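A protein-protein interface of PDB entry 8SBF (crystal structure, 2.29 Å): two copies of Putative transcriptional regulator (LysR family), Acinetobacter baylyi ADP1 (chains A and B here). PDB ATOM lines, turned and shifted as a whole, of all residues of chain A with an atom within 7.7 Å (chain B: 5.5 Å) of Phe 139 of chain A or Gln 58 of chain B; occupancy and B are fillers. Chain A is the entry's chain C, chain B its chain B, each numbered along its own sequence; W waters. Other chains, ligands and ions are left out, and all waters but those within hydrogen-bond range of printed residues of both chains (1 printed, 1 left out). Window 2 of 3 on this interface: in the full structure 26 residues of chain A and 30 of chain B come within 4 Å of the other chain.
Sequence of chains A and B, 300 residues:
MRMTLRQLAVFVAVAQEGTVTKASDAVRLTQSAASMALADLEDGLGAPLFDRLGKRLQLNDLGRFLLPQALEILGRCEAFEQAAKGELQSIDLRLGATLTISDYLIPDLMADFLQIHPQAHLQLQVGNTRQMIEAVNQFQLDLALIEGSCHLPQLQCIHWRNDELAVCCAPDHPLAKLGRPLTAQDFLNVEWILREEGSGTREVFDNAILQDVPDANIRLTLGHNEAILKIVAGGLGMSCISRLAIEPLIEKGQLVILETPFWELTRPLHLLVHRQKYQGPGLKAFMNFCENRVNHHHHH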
ATOM      1  N   ARG A  94      -2.821  -4.036  -1.503  1.00  0.00           N
ATOM      2  CA  ARG A  94      -4.054  -3.262  -1.426  1.00  0.00           C
ATOM      3  C   ARG A  94      -4.996  -3.831  -2.481  1.00  0.00           C
ATOM      4  O   ARG A  94      -4.742  -3.702  -3.683  1.00  0.00           O
ATOM      5  CB  ARG A  94      -3.790  -1.776  -1.657  1.00  0.00           C
ATOM      6  CG  ARG A  94      -2.984  -1.111  -0.550  1.00  0.00           C
ATOM      7  CD  ARG A  94      -2.382   0.203  -1.028  1.00  0.00           C
ATOM      8  NE  ARG A  94      -1.513   0.001  -2.184  1.00  0.00           N
ATOM      9  CZ  ARG A  94      -1.092   0.967  -2.987  1.00  0.00           C
ATOM     10  NH1 ARG A  94      -1.441   2.230  -2.792  1.00  0.00           N
ATOM     11  NH2 ARG A  94      -0.307   0.659  -4.015  1.00  0.00           N
ATOM     12  N   ILE A 133     -11.948   0.526 -11.323  1.00  0.00           N
ATOM     13  CA  ILE A 133     -11.103   0.898 -12.455  1.00  0.00           C
ATOM     14  C   ILE A 133     -10.361   2.192 -12.155  1.00  0.00           C
ATOM     15  O   ILE A 133      -9.159   2.312 -12.421  1.00  0.00           O
ATOM     16  CB  ILE A 133     -11.947   1.012 -13.736  1.00  0.00           C
ATOM     17  CG1 ILE A 133     -12.351  -0.380 -14.224  1.00  0.00           C
ATOM     18  CG2 ILE A 133     -11.176   1.756 -14.816  1.00  0.00           C
ATOM     19  CD1 ILE A 133     -13.781  -0.467 -14.705  1.00  0.00           C
ATOM     20  N   GLU A 134     -11.063   3.181 -11.596  1.00  0.00           N
ATOM     21  CA  GLU A 134     -10.408   4.438 -11.245  1.00  0.00           C
ATOM     22  C   GLU A 134      -9.321   4.215 -10.202  1.00  0.00           C
ATOM     23  O   GLU A 134      -8.222   4.772 -10.310  1.00  0.00           O
ATOM     24  CB  GLU A 134     -11.444   5.443 -10.740  1.00  0.00           C
ATOM     25  CG  GLU A 134     -10.867   6.785 -10.310  1.00  0.00           C
ATOM     26  CD  GLU A 134     -10.212   7.540 -11.451  1.00  0.00           C
ATOM     27  OE1 GLU A 134     -10.314   7.084 -12.610  1.00  0.00           O
ATOM     28  OE2 GLU A 134      -9.593   8.592 -11.186  1.00  0.00           O
ATOM     29  N   ALA A 135      -9.606   3.400  -9.186  1.00  0.00           N
ATOM     30  CA  ALA A 135      -8.604   3.118  -8.162  1.00  0.00           C
ATOM     31  C   ALA A 135      -7.375   2.455  -8.770  1.00  0.00           C
ATOM     32  O   ALA A 135      -6.236   2.837  -8.474  1.00  0.00           O
ATOM     33  CB  ALA A 135      -9.207   2.238  -7.068  1.00  0.00           C
ATOM     34  N   VAL A 136      -7.586   1.455  -9.629  1.00  0.00           N
ATOM     35  CA  VAL A 136      -6.458   0.782 -10.264  1.00  0.00           C
ATOM     36  C   VAL A 136      -5.744   1.719 -11.228  1.00  0.00           C
ATOM     37  O   VAL A 136      -4.519   1.644 -11.386  1.00  0.00           O
ATOM     38  CB  VAL A 136      -6.931  -0.496 -10.981  1.00  0.00           C
ATOM     39  CG1 VAL A 136      -5.758  -1.174 -11.677  1.00  0.00           C
ATOM     40  CG2 VAL A 136      -7.605  -1.442  -9.998  1.00  0.00           C
ATOM     41  N   ASN A 137      -6.486   2.611 -11.890  1.00  0.00           N
ATOM     42  CA  ASN A 137      -5.867   3.514 -12.854  1.00  0.00           C
ATOM     43  C   ASN A 137      -5.019   4.574 -12.162  1.00  0.00           C
ATOM     44  O   ASN A 137      -4.056   5.078 -12.751  1.00  0.00           O
ATOM     45  CB  ASN A 137      -6.943   4.175 -13.715  1.00  0.00           C
ATOM     46  CG  ASN A 137      -6.393   4.722 -15.018  1.00  0.00           C
ATOM     47  OD1 ASN A 137      -5.629   4.051 -15.713  1.00  0.00           O
ATOM     48  ND2 ASN A 137      -6.774   5.949 -15.352  1.00  0.00           N
ATOM     49  N   GLN A 138      -5.358   4.918 -10.922  1.00  0.00           N
ATOM     50  CA  GLN A 138      -4.617   5.903 -10.145  1.00  0.00           C
ATOM     51  C   GLN A 138      -3.472   5.285  -9.349  1.00  0.00           C
ATOM     52  O   GLN A 138      -2.829   5.989  -8.564  1.00  0.00           O
ATOM     53  CB  GLN A 138      -5.566   6.632  -9.188  1.00  0.00           C
ATOM     54  CG  GLN A 138      -6.720   7.354  -9.863  1.00  0.00           C
ATOM     55  CD  GLN A 138      -6.323   8.704 -10.431  1.00  0.00           C
ATOM     56  OE1 GLN A 138      -5.247   9.226 -10.135  1.00  0.00           O
ATOM     57  NE2 GLN A 138      -7.196   9.277 -11.248  1.00  0.00           N
ATOM     58  N   PHE A 139      -3.207   3.990  -9.531  1.00  0.00           N
ATOM     59  CA  PHE A 139      -2.197   3.268  -8.757  1.00  0.00           C
ATOM     60  C   PHE A 139      -2.528   3.255  -7.268  1.00  0.00           C
ATOM     61  O   PHE A 139      -1.632   3.255  -6.421  1.00  0.00           O
ATOM     62  CB  PHE A 139      -0.797   3.852  -8.980  1.00  0.00           C
ATOM     63  CG  PHE A 139      -0.255   3.622 -10.361  1.00  0.00           C
ATOM     64  CD1 PHE A 139      -0.552   4.498 -11.390  1.00  0.00           C
ATOM     65  CD2 PHE A 139       0.560   2.534 -10.630  1.00  0.00           C
ATOM     66  CE1 PHE A 139      -0.052   4.292 -12.661  1.00  0.00           C
ATOM     67  CE2 PHE A 139       1.062   2.323 -11.899  1.00  0.00           C
ATOM     68  CZ  PHE A 139       0.755   3.203 -12.915  1.00  0.00           C
ATOM     69  N   GLN A 140      -3.819   3.246  -6.933  1.00  0.00           N
ATOM     70  CA  GLN A 140      -4.253   3.151  -5.545  1.00  0.00           C
ATOM     71  C   GLN A 140      -4.526   1.720  -5.108  1.00  0.00           C
ATOM     72  O   GLN A 140      -4.629   1.465  -3.904  1.00  0.00           O
ATOM     73  CB  GLN A 140      -5.514   3.996  -5.329  1.00  0.00           C
ATOM     74  CG  GLN A 140      -5.347   5.449  -5.737  1.00  0.00           C
ATOM     75  CD  GLN A 140      -6.554   6.301  -5.398  1.00  0.00           C
ATOM     76  OE1 GLN A 140      -7.643   5.787  -5.142  1.00  0.00           O
ATOM     77  NE2 GLN A 140      -6.365   7.616  -5.391  1.00  0.00           N
ATOM     78  N   LEU A 141      -4.644   0.786  -6.049  1.00  0.00           N
ATOM     79  CA  LEU A 141      -4.836  -0.624  -5.749  1.00  0.00           C
ATOM     80  C   LEU A 141      -3.837  -1.445  -6.546  1.00  0.00           C
ATOM     81  O   LEU A 141      -3.517  -1.109  -7.691  1.00  0.00           O
ATOM     82  CB  LEU A 141      -6.260  -1.084  -6.084  1.00  0.00           C
ATOM     83  CG  LEU A 141      -7.386  -0.649  -5.147  1.00  0.00           C
ATOM     84  CD1 LEU A 141      -8.734  -1.027  -5.747  1.00  0.00           C
ATOM     85  CD2 LEU A 141      -7.222  -1.273  -3.773  1.00  0.00           C
ATOM     86  N   ASP A 142      -3.342  -2.523  -5.936  1.00  0.00           N
ATOM     87  CA  ASP A 142      -2.473  -3.444  -6.656  1.00  0.00           C
ATOM     88  C   ASP A 142      -3.273  -4.403  -7.526  1.00  0.00           C
ATOM     89  O   ASP A 142      -2.793  -4.822  -8.585  1.00  0.00           O
ATOM     90  CB  ASP A 142      -1.613  -4.238  -5.672  1.00  0.00           C
ATOM     91  CG  ASP A 142      -0.844  -3.347  -4.727  1.00  0.00           C
ATOM     92  OD1 ASP A 142      -0.375  -2.277  -5.167  1.00  0.00           O
ATOM     93  OD2 ASP A 142      -0.715  -3.713  -3.540  1.00  0.00           O
ATOM     94  N   GLN A 154      -4.582   0.824 -20.973  1.00  0.00           N
ATOM     95  CA  GLN A 154      -3.485   0.873 -20.013  1.00  0.00           C
ATOM     96  C   GLN A 154      -3.673  -0.116 -18.872  1.00  0.00           C
ATOM     97  O   GLN A 154      -2.699  -0.452 -18.191  1.00  0.00           O
ATOM     98  CB  GLN A 154      -3.317   2.294 -19.458  1.00  0.00           C
ATOM     99  CG  GLN A 154      -4.354   2.738 -18.433  1.00  0.00           C
ATOM    100  CD  GLN A 154      -5.638   3.244 -19.064  1.00  0.00           C
ATOM    101  OE1 GLN A 154      -6.087   2.728 -20.088  1.00  0.00           O
ATOM    102  NE2 GLN A 154      -6.236   4.262 -18.455  1.00  0.00           N
ATOM    103  N   LEU A 155      -4.897  -0.582 -18.646  1.00  0.00           N
ATOM    104  CA  LEU A 155      -5.162  -1.632 -17.677  1.00  0.00           C
ATOM    105  C   LEU A 155      -5.118  -2.992 -18.363  1.00  0.00           C
ATOM    106  O   LEU A 155      -5.394  -3.113 -19.560  1.00  0.00           O
ATOM    107  CB  LEU A 155      -6.526  -1.431 -17.018  1.00  0.00           C
ATOM    108  CG  LEU A 155      -6.820  -0.046 -16.442  1.00  0.00           C
ATOM    109  CD1 LEU A 155      -8.248   0.009 -15.922  1.00  0.00           C
ATOM    110  CD2 LEU A 155      -5.837   0.315 -15.344  1.00  0.00           C
ATOM    111  N   HIS A 274      -2.779  -2.724 -13.348  1.00  0.00           N
ATOM    112  CA  HIS A 274      -2.267  -1.671 -14.215  1.00  0.00           C
ATOM    113  C   HIS A 274      -1.037  -2.183 -14.955  1.00  0.00           C
ATOM    114  O   HIS A 274      -0.091  -2.675 -14.333  1.00  0.00           O
ATOM    115  CB  HIS A 274      -1.923  -0.422 -13.404  1.00  0.00           C
ATOM    116  CG  HIS A 274      -1.868   0.832 -14.218  1.00  0.00           C
ATOM    117  ND1 HIS A 274      -0.956   1.021 -15.234  1.00  0.00           N
ATOM    118  CD2 HIS A 274      -2.609   1.965 -14.163  1.00  0.00           C
ATOM    119  CE1 HIS A 274      -1.140   2.214 -15.773  1.00  0.00           C
ATOM    120  NE2 HIS A 274      -2.136   2.806 -15.141  1.00  0.00           N
ATOM    121  N   ARG A 275      -1.054  -2.062 -16.284  1.00  0.00           N
ATOM    122  CA  ARG A 275       0.015  -2.623 -17.103  1.00  0.00           C
ATOM    123  C   ARG A 275       1.374  -2.012 -16.792  1.00  0.00           C
ATOM    124  O   ARG A 275       2.401  -2.631 -17.092  1.00  0.00           O
ATOM    125  CB  ARG A 275      -0.307  -2.429 -18.585  1.00  0.00           C
ATOM    126  CG  ARG A 275      -1.515  -3.214 -19.062  1.00  0.00           C
ATOM    127  CD  ARG A 275      -1.799  -2.969 -20.539  1.00  0.00           C
ATOM    128  NE  ARG A 275      -2.937  -3.751 -21.009  1.00  0.00           N
ATOM    129  CZ  ARG A 275      -2.856  -4.995 -21.463  1.00  0.00           C
ATOM    130  NH1 ARG A 275      -1.700  -5.637 -21.525  1.00  0.00           N
ATOM    131  NH2 ARG A 275      -3.966  -5.613 -21.861  1.00  0.00           N
ATOM    132  N   GLN A 276       1.407  -0.818 -16.205  1.00  0.00           N
ATOM    133  CA  GLN A 276       2.649  -0.113 -15.923  1.00  0.00           C
ATOM    134  C   GLN A 276       3.086  -0.230 -14.469  1.00  0.00           C
ATOM    135  O   GLN A 276       4.102   0.366 -14.094  1.00  0.00           O
ATOM    136  CB  GLN A 276       2.500   1.367 -16.296  1.00  0.00           C
ATOM    137  CG  GLN A 276       3.135   1.746 -17.622  1.00  0.00           C
ATOM    138  CD  GLN A 276       4.542   2.292 -17.453  1.00  0.00           C
ATOM    139  OE1 GLN A 276       4.766   3.241 -16.700  1.00  0.00           O
ATOM    140  NE2 GLN A 276       5.500   1.692 -18.150  1.00  0.00           N
ATOM    141  N   LYS A 277       2.360  -0.981 -13.649  1.00  0.00           N
ATOM    142  CA  LYS A 277       2.659  -1.106 -12.230  1.00  0.00           C
ATOM    143  C   LYS A 277       3.501  -2.352 -11.991  1.00  0.00           C
ATOM    144  O   LYS A 277       3.136  -3.450 -12.425  1.00  0.00           O
ATOM    145  CB  LYS A 277       1.370  -1.177 -11.411  1.00  0.00           C
ATOM    146  CG  LYS A 277       1.545  -0.850  -9.937  1.00  0.00           C
ATOM    147  CD  LYS A 277       0.216  -0.940  -9.200  1.00  0.00           C
ATOM    148  CE  LYS A 277       0.288  -0.296  -7.824  1.00  0.00           C
ATOM    149  NZ  LYS A 277       1.282  -0.959  -6.933  1.00  0.00           N
ATOM    150  N   TYR A 278       4.630  -2.175 -11.306  1.00  0.00           N
ATOM    151  CA  TYR A 278       5.465  -3.308 -10.938  1.00  0.00           C
ATOM    152  C   TYR A 278       4.662  -4.312 -10.118  1.00  0.00           C
ATOM    153  O   TYR A 278       3.868  -3.940  -9.248  1.00  0.00           O
ATOM    154  CB  TYR A 278       6.682  -2.830 -10.147  1.00  0.00           C
ATOM    155  CG  TYR A 278       7.425  -3.939  -9.439  1.00  0.00           C
ATOM    156  CD1 TYR A 278       8.411  -4.671 -10.088  1.00  0.00           C
ATOM    157  CD2 TYR A 278       7.141  -4.255  -8.116  1.00  0.00           C
ATOM    158  CE1 TYR A 278       9.090  -5.686  -9.441  1.00  0.00           C
ATOM    159  CE2 TYR A 278       7.813  -5.267  -7.462  1.00  0.00           C
ATOM    160  CZ  TYR A 278       8.787  -5.980  -8.129  1.00  0.00           C
ATOM    161  OH  TYR A 278       9.458  -6.989  -7.479  1.00  0.00           O
ATOM    162  N   LEU B  49      12.291   0.869  -8.853  1.00  0.00           N
ATOM    163  CA  LEU B  49      11.922   1.153  -7.474  1.00  0.00           C
ATOM    164  C   LEU B  49      10.707   2.064  -7.358  1.00  0.00           C
ATOM    165  O   LEU B  49      10.141   2.178  -6.264  1.00  0.00           O
ATOM    166  CB  LEU B  49      13.103   1.789  -6.732  1.00  0.00           C
ATOM    167  CG  LEU B  49      14.300   0.872  -6.484  1.00  0.00           C
ATOM    168  CD1 LEU B  49      15.462   1.651  -5.893  1.00  0.00           C
ATOM    169  CD2 LEU B  49      13.910  -0.279  -5.569  1.00  0.00           C
ATOM    170  N   PHE B  50      10.289   2.704  -8.449  1.00  0.00           N
ATOM    171  CA  PHE B  50       9.161   3.622  -8.440  1.00  0.00           C
ATOM    172  C   PHE B  50       8.234   3.324  -9.607  1.00  0.00           C
ATOM    173  O   PHE B  50       8.690   2.986 -10.704  1.00  0.00           O
ATOM    174  CB  PHE B  50       9.627   5.083  -8.526  1.00  0.00           C
ATOM    175  CG  PHE B  50      10.477   5.518  -7.373  1.00  0.00           C
ATOM    176  CD1 PHE B  50       9.897   6.045  -6.231  1.00  0.00           C
ATOM    177  CD2 PHE B  50      11.856   5.403  -7.427  1.00  0.00           C
ATOM    178  CE1 PHE B  50      10.676   6.446  -5.163  1.00  0.00           C
ATOM    179  CE2 PHE B  50      12.640   5.803  -6.363  1.00  0.00           C
ATOM    180  CZ  PHE B  50      12.050   6.324  -5.230  1.00  0.00           C
ATOM    181  N   ASP B  51       6.932   3.451  -9.363  1.00  0.00           N
ATOM    182  CA  ASP B  51       5.952   3.436 -10.439  1.00  0.00           C
ATOM    183  C   ASP B  51       5.842   4.830 -11.044  1.00  0.00           C
ATOM    184  O   ASP B  51       5.861   5.835 -10.326  1.00  0.00           O
ATOM    185  CB  ASP B  51       4.593   2.967  -9.924  1.00  0.00           C
ATOM    186  CG  ASP B  51       4.589   1.498  -9.540  1.00  0.00           C
ATOM    187  OD1 ASP B  51       5.239   0.694 -10.243  1.00  0.00           O
ATOM    188  OD2 ASP B  51       3.939   1.145  -8.533  1.00  0.00           O
ATOM    189  N   ARG B  52       5.734   4.885 -12.366  1.00  0.00           N
ATOM    190  CA  ARG B  52       5.762   6.140 -13.108  1.00  0.00           C
ATOM    191  C   ARG B  52       4.339   6.597 -13.404  1.00  0.00           C
ATOM    192  O   ARG B  52       3.591   5.904 -14.102  1.00  0.00           O
ATOM    193  CB  ARG B  52       6.556   5.978 -14.407  1.00  0.00           C
ATOM    194  CG  ARG B  52       7.997   6.483 -14.351  1.00  0.00           C
ATOM    195  CD  ARG B  52       8.960   5.492 -13.698  1.00  0.00           C
ATOM    196  NE  ARG B  52      10.342   5.951 -13.808  1.00  0.00           N
ATOM    197  CZ  ARG B  52      11.384   5.364 -13.234  1.00  0.00           C
ATOM    198  NH1 ARG B  52      11.244   4.287 -12.477  1.00  0.00           N
ATOM    199  NH2 ARG B  52      12.600   5.872 -13.421  1.00  0.00           N
ATOM    200  N   LEU B  53       3.971   7.764 -12.874  1.00  0.00           N
ATOM    201  CA  LEU B  53       2.675   8.391 -13.115  1.00  0.00           C
ATOM    202  C   LEU B  53       2.824   9.617 -14.014  1.00  0.00           C
ATOM    203  O   LEU B  53       2.131  10.622 -13.849  1.00  0.00           O
ATOM    204  CB  LEU B  53       2.008   8.776 -11.796  1.00  0.00           C
ATOM    205  CG  LEU B  53       1.217   7.681 -11.076  1.00  0.00           C
ATOM    206  CD1 LEU B  53       2.045   6.417 -10.919  1.00  0.00           C
ATOM    207  CD2 LEU B  53       0.733   8.177  -9.718  1.00  0.00           C
ATOM    208  N   ARG B  56       5.475  12.098 -12.143  1.00  0.00           N
ATOM    209  CA  ARG B  56       5.345  11.661 -10.760  1.00  0.00           C
ATOM    210  C   ARG B  56       6.010  10.304 -10.574  1.00  0.00           C
ATOM    211  O   ARG B  56       5.891   9.414 -11.420  1.00  0.00           O
ATOM    212  CB  ARG B  56       3.872  11.557 -10.372  1.00  0.00           C
ATOM    213  CG  ARG B  56       3.280  12.741  -9.621  1.00  0.00           C
ATOM    214  CD  ARG B  56       1.810  12.446  -9.322  1.00  0.00           C
ATOM    215  NE  ARG B  56       1.199  13.345  -8.350  1.00  0.00           N
ATOM    216  CZ  ARG B  56       1.062  13.077  -7.058  1.00  0.00           C
ATOM    217  NH1 ARG B  56       1.553  11.970  -6.523  1.00  0.00           N
ATOM    218  NH2 ARG B  56       0.407  13.938  -6.283  1.00  0.00           N
ATOM    219  N   LEU B  57       6.705  10.144  -9.450  1.00  0.00           N
ATOM    220  CA  LEU B  57       7.282   8.863  -9.060  1.00  0.00           C
ATOM    221  C   LEU B  57       6.798   8.524  -7.660  1.00  0.00           C
ATOM    222  O   LEU B  57       7.064   9.270  -6.711  1.00  0.00           O
ATOM    223  CB  LEU B  57       8.813   8.902  -9.105  1.00  0.00           C
ATOM    224  CG  LEU B  57       9.453   9.020 -10.490  1.00  0.00           C
ATOM    225  CD1 LEU B  57      10.969   9.018 -10.377  1.00  0.00           C
ATOM    226  CD2 LEU B  57       8.988   7.896 -11.398  1.00  0.00           C
ATOM    227  N   GLN B  58       6.082   7.409  -7.531  1.00  0.00           N
ATOM    228  CA  GLN B  58       5.661   6.893  -6.238  1.00  0.00           C
ATOM    229  C   GLN B  58       6.250   5.500  -6.049  1.00  0.00           C
ATOM    230  O   GLN B  58       6.245   4.684  -6.975  1.00  0.00           O
ATOM    231  CB  GLN B  58       4.126   6.859  -6.112  1.00  0.00           C
ATOM    232  CG  GLN B  58       3.432   5.630  -6.675  1.00  0.00           C
ATOM    233  CD  GLN B  58       1.941   5.622  -6.362  1.00  0.00           C
ATOM    234  OE1 GLN B  58       1.302   6.674  -6.305  1.00  0.00           O
ATOM    235  NE2 GLN B  58       1.385   4.434  -6.147  1.00  0.00           N
ATOM    236  N   LEU B  59       6.767   5.247  -4.847  1.00  0.00           N
ATOM    237  CA  LEU B  59       7.373   3.956  -4.540  1.00  0.00           C
ATOM    238  C   LEU B  59       6.466   2.816  -4.979  1.00  0.00           C
ATOM    239  O   LEU B  59       5.243   2.880  -4.831  1.00  0.00           O
ATOM    240  CB  LEU B  59       7.643   3.849  -3.040  1.00  0.00           C
ATOM    241  CG  LEU B  59       8.748   4.723  -2.449  1.00  0.00           C
ATOM    242  CD1 LEU B  59       8.476   4.983  -0.973  1.00  0.00           C
ATOM    243  CD2 LEU B  59      10.101   4.059  -2.631  1.00  0.00           C
ATOM    244  N   ASN B  60       7.073   1.767  -5.527  1.00  0.00           N
ATOM    245  CA  ASN B  60       6.357   0.546  -5.857  1.00  0.00           C
ATOM    246  C   ASN B  60       6.558  -0.474  -4.737  1.00  0.00           C
ATOM    247  O   ASN B  60       7.217  -0.209  -3.729  1.00  0.00           O
ATOM    248  CB  ASN B  60       6.811  -0.002  -7.214  1.00  0.00           C
ATOM    249  CG  ASN B  60       8.282  -0.365  -7.245  1.00  0.00           C
ATOM    250  OD1 ASN B  60       8.910  -0.575  -6.209  1.00  0.00           O
ATOM    251  ND2 ASN B  60       8.837  -0.446  -8.449  1.00  0.00           N
HETATM  252  O   HOH W   1       5.841   2.522 -13.618  1.00  0.00           O
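Hydrophobic or aromatic side chains of chain A that line the printed part of chain B: Phe 139 and Tyr 278.
Hydrophobic or aromatic side chains of chain B that line the printed part of chain A: Leu 53.
Among the printed residues, Asp or Glu carboxylates within 4 Å of a Lys or Arg side-chain nitrogen of the other chain: Lys 277 of chain A with Asp 51 of chain B.
Among the printed residues, merely in contact across the chains: Phe 139 of chain A with Leu 53 of chain B (3.3 Å), Tyr 278 of chain A with Asn 60 of chain B (3.6 Å) and Gln 276 of chain A with Arg 52 of chain B (3.9 Å).
Water W1 bridges the backbone NH (N) of Arg 52 of chain B (2.7 Å) and the backbone carbonyl oxygen (O) of Gln 276 of chain A (2.8 Å).
Of the printed residues of chain B, Phe 139 of chain A touches Leu 53 and Gln 58.
Gln 58 of chain B touches just one residue of chain A: Phe 139.
Of the printed residues of chain B, Lys 277 of chain A touches Asp 51 (3.4 Å).
Of the printed residues of chain B, Tyr 278 of chain A touches Asp 51 and Asn 60.
Of the printed residues of chain A, Asp 51 of chain B touches Lys 277 (3.4 Å) and Tyr 278 (3.1 Å).
The nearest residue of chain A that does not touch Gln 58 of chain B is Arg 94 of chain A (4.7 Å).
No position is printed for both chains.
The side-chain carboxylate of Asp 142 of chain A lies within salt-bridge range of the side-chain amino group of Lys 277 of chain A (2.8 Å).
A ring nitrogen (ND1) of His 274 of chain A lies close to the backbone NH of Gln 276 of chain A (3.1 Å).
The backbone carbonyl oxygen (O) of Leu 49 of chain B lies close to the side-chain amide oxygen (OD1) of Asn 60 of chain B (3.0 Å).
The backbone carbonyl oxygen of Phe 50 of chain B sits at hydrogen-bond distance from the guanidinium group of Arg 52 of chain B, 3.4 Å away.
The side-chain amide nitrogen (ND2) of Asn 60 of chain B sits close to the backbone NH (N) of Phe 50 of chain B (3.5 Å).
The backbone carbonyl oxygen (O) of Gln 58 of chain B lies within hydrogen-bond range of the backbone NH (N) of Asp 51 of chain B (2.8 Å).
The backbone carbonyl oxygen of Phe 139 of chain A is in hydrogen-bond range of the side-chain amide nitrogen of Gln 58 of chain B (3.3 Å).
The side-chain amino group of Lys 277 of chain A is in salt-bridge range of the side-chain carboxylate of Asp 51 of chain B (3.7 Å).
The backbone NH (N) of Tyr 278 of chain A sits at hydrogen-bond distance from the side-chain carboxylate (OD1) of Asp 51 of chain B (3.1 Å).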
